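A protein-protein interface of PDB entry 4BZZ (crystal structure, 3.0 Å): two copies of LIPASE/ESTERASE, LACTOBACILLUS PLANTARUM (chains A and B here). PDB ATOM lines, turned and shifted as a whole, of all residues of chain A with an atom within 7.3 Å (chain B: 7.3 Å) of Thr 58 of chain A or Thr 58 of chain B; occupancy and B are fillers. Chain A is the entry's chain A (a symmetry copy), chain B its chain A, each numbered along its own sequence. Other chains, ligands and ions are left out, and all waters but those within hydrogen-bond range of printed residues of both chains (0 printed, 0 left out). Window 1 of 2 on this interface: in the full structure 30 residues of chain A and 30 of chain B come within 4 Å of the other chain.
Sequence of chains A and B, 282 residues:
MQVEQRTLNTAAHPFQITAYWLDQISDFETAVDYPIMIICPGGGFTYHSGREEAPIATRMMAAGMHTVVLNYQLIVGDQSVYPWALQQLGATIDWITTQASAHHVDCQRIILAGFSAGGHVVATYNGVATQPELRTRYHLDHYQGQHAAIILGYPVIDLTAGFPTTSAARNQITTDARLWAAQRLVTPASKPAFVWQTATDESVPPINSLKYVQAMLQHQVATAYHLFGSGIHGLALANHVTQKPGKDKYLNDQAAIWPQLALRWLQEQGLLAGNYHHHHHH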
ATOM      1  N   MET A   1      17.864 -27.557  25.386  1.00  0.00           N
ATOM      2  CA  MET A   1      18.158 -26.777  24.191  1.00  0.00           C
ATOM      3  C   MET A   1      18.994 -27.589  23.208  1.00  0.00           C
ATOM      4  O   MET A   1      19.983 -28.212  23.586  1.00  0.00           O
ATOM      5  CB  MET A   1      18.887 -25.485  24.557  1.00  0.00           C
ATOM      6  CG  MET A   1      19.165 -24.572  23.366  1.00  0.00           C
ATOM      7  SD  MET A   1      20.450 -23.355  23.746  1.00  0.00           S
ATOM      8  CE  MET A   1      19.864 -22.757  25.329  1.00  0.00           C
ATOM      9  N   TYR A  20      18.545 -22.734  16.796  1.00  0.00           N
ATOM     10  CA  TYR A  20      18.640 -22.941  18.238  1.00  0.00           C
ATOM     11  C   TYR A  20      17.252 -23.286  18.758  1.00  0.00           C
ATOM     12  O   TYR A  20      16.400 -22.411  18.885  1.00  0.00           O
ATOM     13  CB  TYR A  20      19.200 -21.695  18.936  1.00  0.00           C
ATOM     14  CG  TYR A  20      20.627 -21.335  18.530  1.00  0.00           C
ATOM     15  CD1 TYR A  20      21.710 -21.874  19.189  1.00  0.00           C
ATOM     16  CD2 TYR A  20      20.879 -20.447  17.494  1.00  0.00           C
ATOM     17  CE1 TYR A  20      22.999 -21.553  18.831  1.00  0.00           C
ATOM     18  CE2 TYR A  20      22.171 -20.123  17.123  1.00  0.00           C
ATOM     19  CZ  TYR A  20      23.226 -20.683  17.795  1.00  0.00           C
ATOM     20  OH  TYR A  20      24.521 -20.369  17.437  1.00  0.00           O
ATOM     21  N   LEU A  22      14.327 -24.501  21.337  1.00  0.00           N
ATOM     22  CA  LEU A  22      13.917 -24.613  22.740  1.00  0.00           C
ATOM     23  C   LEU A  22      13.438 -26.037  23.044  1.00  0.00           C
ATOM     24  O   LEU A  22      12.731 -26.660  22.234  1.00  0.00           O
ATOM     25  CB  LEU A  22      12.792 -23.643  23.046  1.00  0.00           C
ATOM     26  CG  LEU A  22      13.102 -22.395  23.851  1.00  0.00           C
ATOM     27  CD1 LEU A  22      14.473 -21.869  23.535  1.00  0.00           C
ATOM     28  CD2 LEU A  22      12.041 -21.334  23.584  1.00  0.00           C
ATOM     29  N   ILE A  39      16.905 -14.713  11.949  1.00  0.00           N
ATOM     30  CA  ILE A  39      17.823 -13.591  12.072  1.00  0.00           C
ATOM     31  C   ILE A  39      18.766 -13.533  10.882  1.00  0.00           C
ATOM     32  O   ILE A  39      19.415 -14.531  10.532  1.00  0.00           O
ATOM     33  CB  ILE A  39      18.671 -13.667  13.352  1.00  0.00           C
ATOM     34  CG1 ILE A  39      17.780 -13.811  14.593  1.00  0.00           C
ATOM     35  CG2 ILE A  39      19.543 -12.430  13.475  1.00  0.00           C
ATOM     36  CD1 ILE A  39      18.541 -14.097  15.860  1.00  0.00           C
ATOM     37  N   GLU A  53      24.603 -12.470  15.345  1.00  0.00           N
ATOM     38  CA  GLU A  53      24.015 -13.806  15.281  1.00  0.00           C
ATOM     39  C   GLU A  53      23.692 -14.375  16.673  1.00  0.00           C
ATOM     40  O   GLU A  53      22.651 -14.063  17.242  1.00  0.00           O
ATOM     41  CB  GLU A  53      24.913 -14.746  14.479  1.00  0.00           C
ATOM     42  CG  GLU A  53      24.978 -14.401  13.004  1.00  0.00           C
ATOM     43  CD  GLU A  53      26.101 -15.115  12.279  1.00  0.00           C
ATOM     44  OE1 GLU A  53      27.241 -15.104  12.786  1.00  0.00           O
ATOM     45  OE2 GLU A  53      25.848 -15.681  11.193  1.00  0.00           O
ATOM     46  N   ALA A  54      24.581 -15.197  17.227  1.00  0.00           N
ATOM     47  CA  ALA A  54      24.318 -15.820  18.528  1.00  0.00           C
ATOM     48  C   ALA A  54      24.054 -14.863  19.733  1.00  0.00           C
ATOM     49  O   ALA A  54      23.155 -15.124  20.541  1.00  0.00           O
ATOM     50  CB  ALA A  54      25.372 -16.839  18.849  1.00  0.00           C
ATOM     51  N   PRO A  55      24.807 -13.752  19.857  1.00  0.00           N
ATOM     52  CA  PRO A  55      24.457 -12.845  20.955  1.00  0.00           C
ATOM     53  C   PRO A  55      23.016 -12.367  20.914  1.00  0.00           C
ATOM     54  O   PRO A  55      22.395 -12.227  21.965  1.00  0.00           O
ATOM     55  CB  PRO A  55      25.399 -11.665  20.735  1.00  0.00           C
ATOM     56  CG  PRO A  55      26.603 -12.286  20.152  1.00  0.00           C
ATOM     57  CD  PRO A  55      26.069 -13.345  19.216  1.00  0.00           C
ATOM     58  N   ILE A  56      22.492 -12.128  19.720  1.00  0.00           N
ATOM     59  CA  ILE A  56      21.121 -11.673  19.571  1.00  0.00           C
ATOM     60  C   ILE A  56      20.159 -12.848  19.711  1.00  0.00           C
ATOM     61  O   ILE A  56      19.165 -12.765  20.446  1.00  0.00           O
ATOM     62  CB  ILE A  56      20.935 -10.976  18.218  1.00  0.00           C
ATOM     63  CG1 ILE A  56      21.873  -9.777  18.142  1.00  0.00           C
ATOM     64  CG2 ILE A  56      19.499 -10.529  18.021  1.00  0.00           C
ATOM     65  CD1 ILE A  56      21.679  -8.951  16.924  1.00  0.00           C
ATOM     66  N   ALA A  57      20.482 -13.941  19.017  1.00  0.00           N
ATOM     67  CA  ALA A  57      19.716 -15.185  19.075  1.00  0.00           C
ATOM     68  C   ALA A  57      19.467 -15.591  20.501  1.00  0.00           C
ATOM     69  O   ALA A  57      18.317 -15.817  20.883  1.00  0.00           O
ATOM     70  CB  ALA A  57      20.440 -16.291  18.355  1.00  0.00           C
ATOM     71  N   THR A  58      20.544 -15.672  21.285  1.00  0.00           N
ATOM     72  CA  THR A  58      20.456 -16.041  22.700  1.00  0.00           C
ATOM     73  C   THR A  58      19.571 -15.082  23.470  1.00  0.00           C
ATOM     74  O   THR A  58      18.791 -15.508  24.332  1.00  0.00           O
ATOM     75  CB  THR A  58      21.835 -16.053  23.372  1.00  0.00           C
ATOM     76  OG1 THR A  58      22.729 -16.891  22.627  1.00  0.00           O
ATOM     77  CG2 THR A  58      21.732 -16.574  24.791  1.00  0.00           C
ATOM     78  N   ARG A  59      19.678 -13.790  23.156  1.00  0.00           N
ATOM     79  CA  ARG A  59      18.871 -12.782  23.855  1.00  0.00           C
ATOM     80  C   ARG A  59      17.372 -13.022  23.661  1.00  0.00           C
ATOM     81  O   ARG A  59      16.583 -12.886  24.600  1.00  0.00           O
ATOM     82  CB  ARG A  59      19.244 -11.344  23.445  1.00  0.00           C
ATOM     83  CG  ARG A  59      18.475 -10.276  24.235  1.00  0.00           C
ATOM     84  CD  ARG A  59      18.484 -10.638  25.724  1.00  0.00           C
ATOM     85  NE  ARG A  59      17.745  -9.720  26.594  1.00  0.00           N
ATOM     86  CZ  ARG A  59      16.537  -9.978  27.083  1.00  0.00           C
ATOM     87  NH1 ARG A  59      15.929 -11.114  26.772  1.00  0.00           N
ATOM     88  NH2 ARG A  59      15.935  -9.110  27.885  1.00  0.00           N
ATOM     89  N   MET A  60      16.992 -13.380  22.440  1.00  0.00           N
ATOM     90  CA  MET A  60      15.598 -13.624  22.137  1.00  0.00           C
ATOM     91  C   MET A  60      15.127 -14.963  22.703  1.00  0.00           C
ATOM     92  O   MET A  60      13.988 -15.084  23.160  1.00  0.00           O
ATOM     93  CB  MET A  60      15.375 -13.551  20.628  1.00  0.00           C
ATOM     94  CG  MET A  60      15.798 -12.217  20.033  1.00  0.00           C
ATOM     95  SD  MET A  60      14.905 -10.800  20.718  1.00  0.00           S
ATOM     96  CE  MET A  60      15.873  -9.440  20.083  1.00  0.00           C
ATOM     97  N   MET A  61      16.009 -15.963  22.666  1.00  0.00           N
ATOM     98  CA  MET A  61      15.738 -17.267  23.267  1.00  0.00           C
ATOM     99  C   MET A  61      15.373 -17.140  24.740  1.00  0.00           C
ATOM    100  O   MET A  61      14.474 -17.833  25.219  1.00  0.00           O
ATOM    101  CB  MET A  61      16.939 -18.191  23.123  1.00  0.00           C
ATOM    102  CG  MET A  61      16.896 -19.095  21.897  1.00  0.00           C
ATOM    103  SD  MET A  61      17.772 -20.668  22.160  1.00  0.00           S
ATOM    104  CE  MET A  61      19.409 -20.061  22.564  1.00  0.00           C
ATOM    105  N   ALA A  62      16.064 -16.245  25.449  1.00  0.00           N
ATOM    106  CA  ALA A  62      15.774 -15.986  26.861  1.00  0.00           C
ATOM    107  C   ALA A  62      14.327 -15.548  27.106  1.00  0.00           C
ATOM    108  O   ALA A  62      13.789 -15.710  28.205  1.00  0.00           O
ATOM    109  CB  ALA A  62      16.737 -14.956  27.426  1.00  0.00           C
ATOM    110  N   ALA A  63      13.699 -14.988  26.081  1.00  0.00           N
ATOM    111  CA  ALA A  63      12.313 -14.564  26.195  1.00  0.00           C
ATOM    112  C   ALA A  63      11.362 -15.665  25.741  1.00  0.00           C
ATOM    113  O   ALA A  63      10.160 -15.442  25.628  1.00  0.00           O
ATOM    114  CB  ALA A  63      12.068 -13.285  25.411  1.00  0.00           C
ATOM    115  N   GLY A  64      11.901 -16.850  25.475  1.00  0.00           N
ATOM    116  CA  GLY A  64      11.067 -18.004  25.206  1.00  0.00           C
ATOM    117  C   GLY A  64      10.606 -18.148  23.771  1.00  0.00           C
ATOM    118  O   GLY A  64       9.411 -18.282  23.501  1.00  0.00           O
ATOM    119  N   MET A  65      11.565 -18.117  22.850  1.00  0.00           N
ATOM    120  CA  MET A  65      11.307 -18.395  21.448  1.00  0.00           C
ATOM    121  C   MET A  65      12.493 -19.123  20.820  1.00  0.00           C
ATOM    122  O   MET A  65      13.635 -18.896  21.195  1.00  0.00           O
ATOM    123  CB  MET A  65      10.994 -17.102  20.695  1.00  0.00           C
ATOM    124  CG  MET A  65      12.072 -16.039  20.763  1.00  0.00           C
ATOM    125  SD  MET A  65      11.651 -14.539  19.824  1.00  0.00           S
ATOM    126  CE  MET A  65      10.252 -13.942  20.742  1.00  0.00           C
ATOM    127  N   THR A  67      15.123 -19.752  17.797  1.00  0.00           N
ATOM    128  CA  THR A  67      15.725 -18.871  16.790  1.00  0.00           C
ATOM    129  C   THR A  67      16.458 -19.645  15.690  1.00  0.00           C
ATOM    130  O   THR A  67      17.054 -20.695  15.935  1.00  0.00           O
ATOM    131  CB  THR A  67      16.691 -17.833  17.406  1.00  0.00           C
ATOM    132  OG1 THR A  67      17.725 -18.509  18.130  1.00  0.00           O
ATOM    133  CG2 THR A  67      15.954 -16.878  18.335  1.00  0.00           C
ATOM    134  N   LEU A 237      23.867  -5.545  20.319  1.00  0.00           N
ATOM    135  CA  LEU A 237      23.236  -5.528  21.637  1.00  0.00           C
ATOM    136  C   LEU A 237      23.567  -4.244  22.410  1.00  0.00           C
ATOM    137  O   LEU A 237      22.953  -3.970  23.440  1.00  0.00           O
ATOM    138  CB  LEU A 237      23.613  -6.776  22.445  1.00  0.00           C
ATOM    139  CG  LEU A 237      22.881  -8.083  22.105  1.00  0.00           C
ATOM    140  CD1 LEU A 237      23.383  -9.262  22.934  1.00  0.00           C
ATOM    141  CD2 LEU A 237      21.391  -7.938  22.286  1.00  0.00           C
ATOM    142  N   MET B   1      27.330 -21.381  19.585  1.00  0.00           N
ATOM    143  CA  MET B   1      26.971 -21.986  20.860  1.00  0.00           C
ATOM    144  C   MET B   1      26.996 -23.507  20.764  1.00  0.00           C
ATOM    145  O   MET B   1      26.450 -24.088  19.828  1.00  0.00           O
ATOM    146  CB  MET B   1      25.590 -21.512  21.313  1.00  0.00           C
ATOM    147  CG  MET B   1      25.171 -22.040  22.681  1.00  0.00           C
ATOM    148  SD  MET B   1      23.385 -21.896  22.932  1.00  0.00           S
ATOM    149  CE  MET B   1      23.126 -20.202  22.409  1.00  0.00           C
ATOM    150  N   TYR B  20      26.324 -25.322  28.583  1.00  0.00           N
ATOM    151  CA  TYR B  20      25.996 -24.485  27.433  1.00  0.00           C
ATOM    152  C   TYR B  20      27.162 -23.536  27.192  1.00  0.00           C
ATOM    153  O   TYR B  20      27.332 -22.562  27.921  1.00  0.00           O
ATOM    154  CB  TYR B  20      24.692 -23.713  27.669  1.00  0.00           C
ATOM    155  CG  TYR B  20      23.458 -24.597  27.832  1.00  0.00           C
ATOM    156  CD1 TYR B  20      22.721 -24.996  26.739  1.00  0.00           C
ATOM    157  CD2 TYR B  20      23.034 -25.017  29.084  1.00  0.00           C
ATOM    158  CE1 TYR B  20      21.607 -25.791  26.878  1.00  0.00           C
ATOM    159  CE2 TYR B  20      21.919 -25.822  29.233  1.00  0.00           C
ATOM    160  CZ  TYR B  20      21.212 -26.207  28.124  1.00  0.00           C
ATOM    161  OH  TYR B  20      20.097 -27.008  28.256  1.00  0.00           O
ATOM    162  N   LEU B  22      29.509 -20.755  25.338  1.00  0.00           N
ATOM    163  CA  LEU B  22      29.543 -19.623  24.407  1.00  0.00           C
ATOM    164  C   LEU B  22      30.627 -19.839  23.344  1.00  0.00           C
ATOM    165  O   LEU B  22      31.737 -20.308  23.649  1.00  0.00           O
ATOM    166  CB  LEU B  22      29.835 -18.332  25.148  1.00  0.00           C
ATOM    167  CG  LEU B  22      28.701 -17.349  25.375  1.00  0.00           C
ATOM    168  CD1 LEU B  22      27.400 -18.061  25.605  1.00  0.00           C
ATOM    169  CD2 LEU B  22      29.037 -16.441  26.554  1.00  0.00           C
ATOM    170  N   ILE B  39      24.478 -23.890  37.806  1.00  0.00           N
ATOM    171  CA  ILE B  39      23.101 -23.767  38.260  1.00  0.00           C
ATOM    172  C   ILE B  39      22.618 -25.070  38.873  1.00  0.00           C
ATOM    173  O   ILE B  39      22.732 -26.145  38.263  1.00  0.00           O
ATOM    174  CB  ILE B  39      22.141 -23.389  37.119  1.00  0.00           C
ATOM    175  CG1 ILE B  39      22.618 -22.121  36.398  1.00  0.00           C
ATOM    176  CG2 ILE B  39      20.739 -23.185  37.663  1.00  0.00           C
ATOM    177  CD1 ILE B  39      21.846 -21.805  35.145  1.00  0.00           C
ATOM    178  N   GLU B  53      16.246 -24.686  35.079  1.00  0.00           N
ATOM    179  CA  GLU B  53      17.462 -25.051  34.356  1.00  0.00           C
ATOM    180  C   GLU B  53      17.679 -24.195  33.097  1.00  0.00           C
ATOM    181  O   GLU B  53      18.196 -23.086  33.186  1.00  0.00           O
ATOM    182  CB  GLU B  53      17.461 -26.545  34.032  1.00  0.00           C
ATOM    183  CG  GLU B  53      17.594 -27.426  35.258  1.00  0.00           C
ATOM    184  CD  GLU B  53      17.270 -28.879  34.980  1.00  0.00           C
ATOM    185  OE1 GLU B  53      16.226 -29.150  34.353  1.00  0.00           O
ATOM    186  OE2 GLU B  53      18.055 -29.758  35.398  1.00  0.00           O
ATOM    187  N   ALA B  54      17.277 -24.696  31.930  1.00  0.00           N
ATOM    188  CA  ALA B  54      17.500 -23.960  30.682  1.00  0.00           C
ATOM    189  C   ALA B  54      16.883 -22.529  30.582  1.00  0.00           C
ATOM    190  O   ALA B  54      17.539 -21.610  30.078  1.00  0.00           O
ATOM    191  CB  ALA B  54      17.132 -24.806  29.497  1.00  0.00           C
ATOM    192  N   PRO B  55      15.643 -22.321  31.069  1.00  0.00           N
ATOM    193  CA  PRO B  55      15.150 -20.940  31.030  1.00  0.00           C
ATOM    194  C   PRO B  55      16.050 -19.952  31.750  1.00  0.00           C
ATOM    195  O   PRO B  55      16.203 -18.824  31.285  1.00  0.00           O
ATOM    196  CB  PRO B  55      13.809 -21.038  31.751  1.00  0.00           C
ATOM    197  CG  PRO B  55      13.334 -22.394  31.418  1.00  0.00           C
ATOM    198  CD  PRO B  55      14.575 -23.254  31.466  1.00  0.00           C
ATOM    199  N   ILE B  56      16.640 -20.369  32.862  1.00  0.00           N
ATOM    200  CA  ILE B  56      17.524 -19.504  33.622  1.00  0.00           C
ATOM    201  C   ILE B  56      18.899 -19.448  32.963  1.00  0.00           C
ATOM    202  O   ILE B  56      19.461 -18.360  32.770  1.00  0.00           O
ATOM    203  CB  ILE B  56      17.634 -19.995  35.070  1.00  0.00           C
ATOM    204  CG1 ILE B  56      16.248 -19.982  35.707  1.00  0.00           C
ATOM    205  CG2 ILE B  56      18.586 -19.129  35.874  1.00  0.00           C
ATOM    206  CD1 ILE B  56      16.261 -20.312  37.153  1.00  0.00           C
ATOM    207  N   ALA B  57      19.414 -20.626  32.606  1.00  0.00           N
ATOM    208  CA  ALA B  57      20.689 -20.766  31.907  1.00  0.00           C
ATOM    209  C   ALA B  57      20.750 -19.847  30.718  1.00  0.00           C
ATOM    210  O   ALA B  57      21.695 -19.067  30.593  1.00  0.00           O
ATOM    211  CB  ALA B  57      20.898 -22.187  31.457  1.00  0.00           C
ATOM    212  N   THR B  58      19.735 -19.937  29.856  1.00  0.00           N
ATOM    213  CA  THR B  58      19.649 -19.097  28.659  1.00  0.00           C
ATOM    214  C   THR B  58      19.638 -17.623  29.015  1.00  0.00           C
ATOM    215  O   THR B  58      20.275 -16.812  28.331  1.00  0.00           O
ATOM    216  CB  THR B  58      18.384 -19.395  27.843  1.00  0.00           C
ATOM    217  OG1 THR B  58      18.317 -20.797  27.551  1.00  0.00           O
ATOM    218  CG2 THR B  58      18.392 -18.617  26.543  1.00  0.00           C
ATOM    219  N   ARG B  59      18.926 -17.275  30.088  1.00  0.00           N
ATOM    220  CA  ARG B  59      18.843 -15.870  30.506  1.00  0.00           C
ATOM    221  C   ARG B  59      20.220 -15.300  30.853  1.00  0.00           C
ATOM    222  O   ARG B  59      20.539 -14.160  30.504  1.00  0.00           O
ATOM    223  CB  ARG B  59      17.864 -15.663  31.677  1.00  0.00           C
ATOM    224  CG  ARG B  59      17.695 -14.188  32.064  1.00  0.00           C
ATOM    225  CD  ARG B  59      17.509 -13.346  30.798  1.00  0.00           C
ATOM    226  NE  ARG B  59      17.378 -11.904  31.020  1.00  0.00           N
ATOM    227  CZ  ARG B  59      18.360 -11.034  30.815  1.00  0.00           C
ATOM    228  NH1 ARG B  59      19.544 -11.462  30.402  1.00  0.00           N
ATOM    229  NH2 ARG B  59      18.163  -9.737  31.015  1.00  0.00           N
ATOM    230  N   MET B  60      21.029 -16.103  31.536  1.00  0.00           N
ATOM    231  CA  MET B  60      22.352 -15.666  31.929  1.00  0.00           C
ATOM    232  C   MET B  60      23.315 -15.666  30.743  1.00  0.00           C
ATOM    233  O   MET B  60      24.177 -14.789  30.636  1.00  0.00           O
ATOM    234  CB  MET B  60      22.871 -16.543  33.065  1.00  0.00           C
ATOM    235  CG  MET B  60      21.955 -16.541  34.279  1.00  0.00           C
ATOM    236  SD  MET B  60      21.721 -14.902  35.008  1.00  0.00           S
ATOM    237  CE  MET B  60      20.366 -15.211  36.130  1.00  0.00           C
ATOM    238  N   MET B  61      23.167 -16.653  29.860  1.00  0.00           N
ATOM    239  CA  MET B  61      23.944 -16.722  28.624  1.00  0.00           C
ATOM    240  C   MET B  61      23.793 -15.451  27.798  1.00  0.00           C
ATOM    241  O   MET B  61      24.769 -14.965  27.223  1.00  0.00           O
ATOM    242  CB  MET B  61      23.525 -17.921  27.785  1.00  0.00           C
ATOM    243  CG  MET B  61      24.363 -19.173  28.013  1.00  0.00           C
ATOM    244  SD  MET B  61      24.457 -20.228  26.534  1.00  0.00           S
ATOM    245  CE  MET B  61      22.715 -20.552  26.260  1.00  0.00           C
ATOM    246  N   ALA B  62      22.573 -14.911  27.752  1.00  0.00           N
ATOM    247  CA  ALA B  62      22.307 -13.660  27.040  1.00  0.00           C
ATOM    248  C   ALA B  62      23.161 -12.491  27.539  1.00  0.00           C
ATOM    249  O   ALA B  62      23.401 -11.522  26.814  1.00  0.00           O
ATOM    250  CB  ALA B  62      20.832 -13.303  27.117  1.00  0.00           C
ATOM    251  N   ALA B  63      23.615 -12.582  28.782  1.00  0.00           N
ATOM    252  CA  ALA B  63      24.462 -11.542  29.344  1.00  0.00           C
ATOM    253  C   ALA B  63      25.937 -11.863  29.140  1.00  0.00           C
ATOM    254  O   ALA B  63      26.804 -11.178  29.674  1.00  0.00           O
ATOM    255  CB  ALA B  63      24.157 -11.331  30.819  1.00  0.00           C
ATOM    256  N   GLY B  64      26.221 -12.911  28.372  1.00  0.00           N
ATOM    257  CA  GLY B  64      27.586 -13.195  27.976  1.00  0.00           C
ATOM    258  C   GLY B  64      28.396 -13.996  28.973  1.00  0.00           C
ATOM    259  O   GLY B  64      29.491 -13.593  29.368  1.00  0.00           O
ATOM    260  N   MET B  65      27.846 -15.136  29.380  1.00  0.00           N
ATOM    261  CA  MET B  65      28.558 -16.090  30.213  1.00  0.00           C
ATOM    262  C   MET B  65      28.168 -17.520  29.842  1.00  0.00           C
ATOM    263  O   MET B  65      27.037 -17.776  29.453  1.00  0.00           O
ATOM    264  CB  MET B  65      28.292 -15.815  31.692  1.00  0.00           C
ATOM    265  CG  MET B  65      26.834 -15.845  32.102  1.00  0.00           C
ATOM    266  SD  MET B  65      26.588 -15.537  33.878  1.00  0.00           S
ATOM    267  CE  MET B  65      27.147 -13.856  34.014  1.00  0.00           C
ATOM    268  N   THR B  67      27.175 -21.331  30.810  1.00  0.00           N
ATOM    269  CA  THR B  67      26.468 -21.926  31.949  1.00  0.00           C
ATOM    270  C   THR B  67      26.583 -23.454  31.983  1.00  0.00           C
ATOM    271  O   THR B  67      26.619 -24.117  30.946  1.00  0.00           O
ATOM    272  CB  THR B  67      24.974 -21.533  31.996  1.00  0.00           C
ATOM    273  OG1 THR B  67      24.333 -21.926  30.777  1.00  0.00           O
ATOM    274  CG2 THR B  67      24.805 -20.034  32.203  1.00  0.00           C
ATOM    275  N   LEU B 237      11.795 -17.542  36.619  1.00  0.00           N
ATOM    276  CA  LEU B 237      11.956 -16.285  35.890  1.00  0.00           C
ATOM    277  C   LEU B 237      10.796 -15.318  36.159  1.00  0.00           C
ATOM    278  O   LEU B 237      10.875 -14.144  35.799  1.00  0.00           O
ATOM    279  CB  LEU B 237      12.132 -16.537  34.388  1.00  0.00           C
ATOM    280  CG  LEU B 237      13.517 -16.999  33.908  1.00  0.00           C
ATOM    281  CD1 LEU B 237      13.550 -17.273  32.407  1.00  0.00           C
ATOM    282  CD2 LEU B 237      14.582 -15.992  34.261  1.00  0.00           C
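The side-chain sulfur (SD) of Met 1 of chain A lies close to the side-chain sulfur (SD) of Met 1 of chain B (3.4 Å).
The backbone NH (N) of Tyr 20 of chain B sits at hydrogen-bond distance from the backbone carbonyl oxygen (O) of Thr 67 of chain B.
The backbone carbonyl oxygen (O) of Ala 54 of chain B sits at hydrogen-bond distance from the side-chain hydroxyl (OG1) of Thr 58 of chain B (2.8 Å).
N of Tyr 20 of chain A lies within hydrogen-bond range of O of Thr 67 of chain A (2.7 Å).
The backbone carbonyl oxygen of Ala 54 of chain A sits at hydrogen-bond distance from the side-chain hydroxyl of Thr 58 of chain A, at 2.8 Å.
Met 1 of chain A touches Tyr 20 of chain B (CB to CE1, 3.6 Å).
Thr 58 of chain B touches Met 1 of chain A (OG1 to CE, 3.3 Å).
Met 1 of chain B touches Tyr 20 of chain A (CB to CE1, 3.6 Å).
CG2 of Thr 58 of chain A touches O of Thr 58 of chain B (3.8 Å).
Thr 58 of chain A touches Met 61 of chain B.
Ala 62 of chain B touches Thr 58 of chain A.
Arg 59 of chain A touches Ala 62 of chain B (CD to CB, 3.8 Å).
CB of Met 61 of chain A touches CG2 of Thr 58 of chain B, 3.7 Å away.
Thr 58 of chain B touches Ala 62 of chain A (CG2 to N, 3.5 Å).
CB of Ala 62 of chain A touches CD of Arg 59 of chain B, 3.8 Å away.
Of chain B, only Met 1 (3.3 Å), Thr 58 (3.8 Å), Met 61 (3.7 Å) and Ala 62 (3.5 Å) come within 4 Å of Thr 58 of chain A.
No residue of chain A comes within 4 Å of Ala 57 of chain B.
Printed residues of chain A within 4 Å of Met 61 of chain B: Met 1 and Thr 58.
Printed residues of chain A within 4 Å of Met 1 of chain B: Met 1 (3.4 Å), Tyr 20 (3.6 Å), Thr 58 (3.3 Å) and Met 61 (3.7 Å).
Leu 22 of chain B touches none of the printed residues of chain A.
The nearest residue of chain A that does not touch Thr 58 of chain B is Leu 22 of chain A (5.7 Å).
The nearest printed residue of chain B that does not touch Arg 59 of chain A is Thr 58 of chain B (6.0 Å).
Hydrophobic or aromatic side chains of chain A within 4 Å of the printed part of chain B: Met 1, Tyr 20, Met 61 and Ala 62.
Among the printed residues, 15 pairs touch across the chains.
Met 1 of chain A touches Thr 58 of chain B, and with the chains exchanged Thr 58 of chain A touches Met 1 of chain B.
Met 1 of chain A touches Met 61 of chain B, and with the chains exchanged Met 61 of chain A touches Met 1 of chain B.
Thr 58 of chain A touches Met 61 of chain B, and with the chains exchanged Met 61 of chain A touches Thr 58 of chain B.
Arg 59 of chain A touches its own counterpart, Arg 59 of chain B.
Positions printed for both chains: 1, 20, 22, 39, 53, 54, 55, 56, 57, 58, 59, 60, 61, 62, 63, 64, 65, 67 and 237.
Of the 15 pairs that touch across the chains among the printed residues, 15 have their exchanged pair printed and touching as well.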
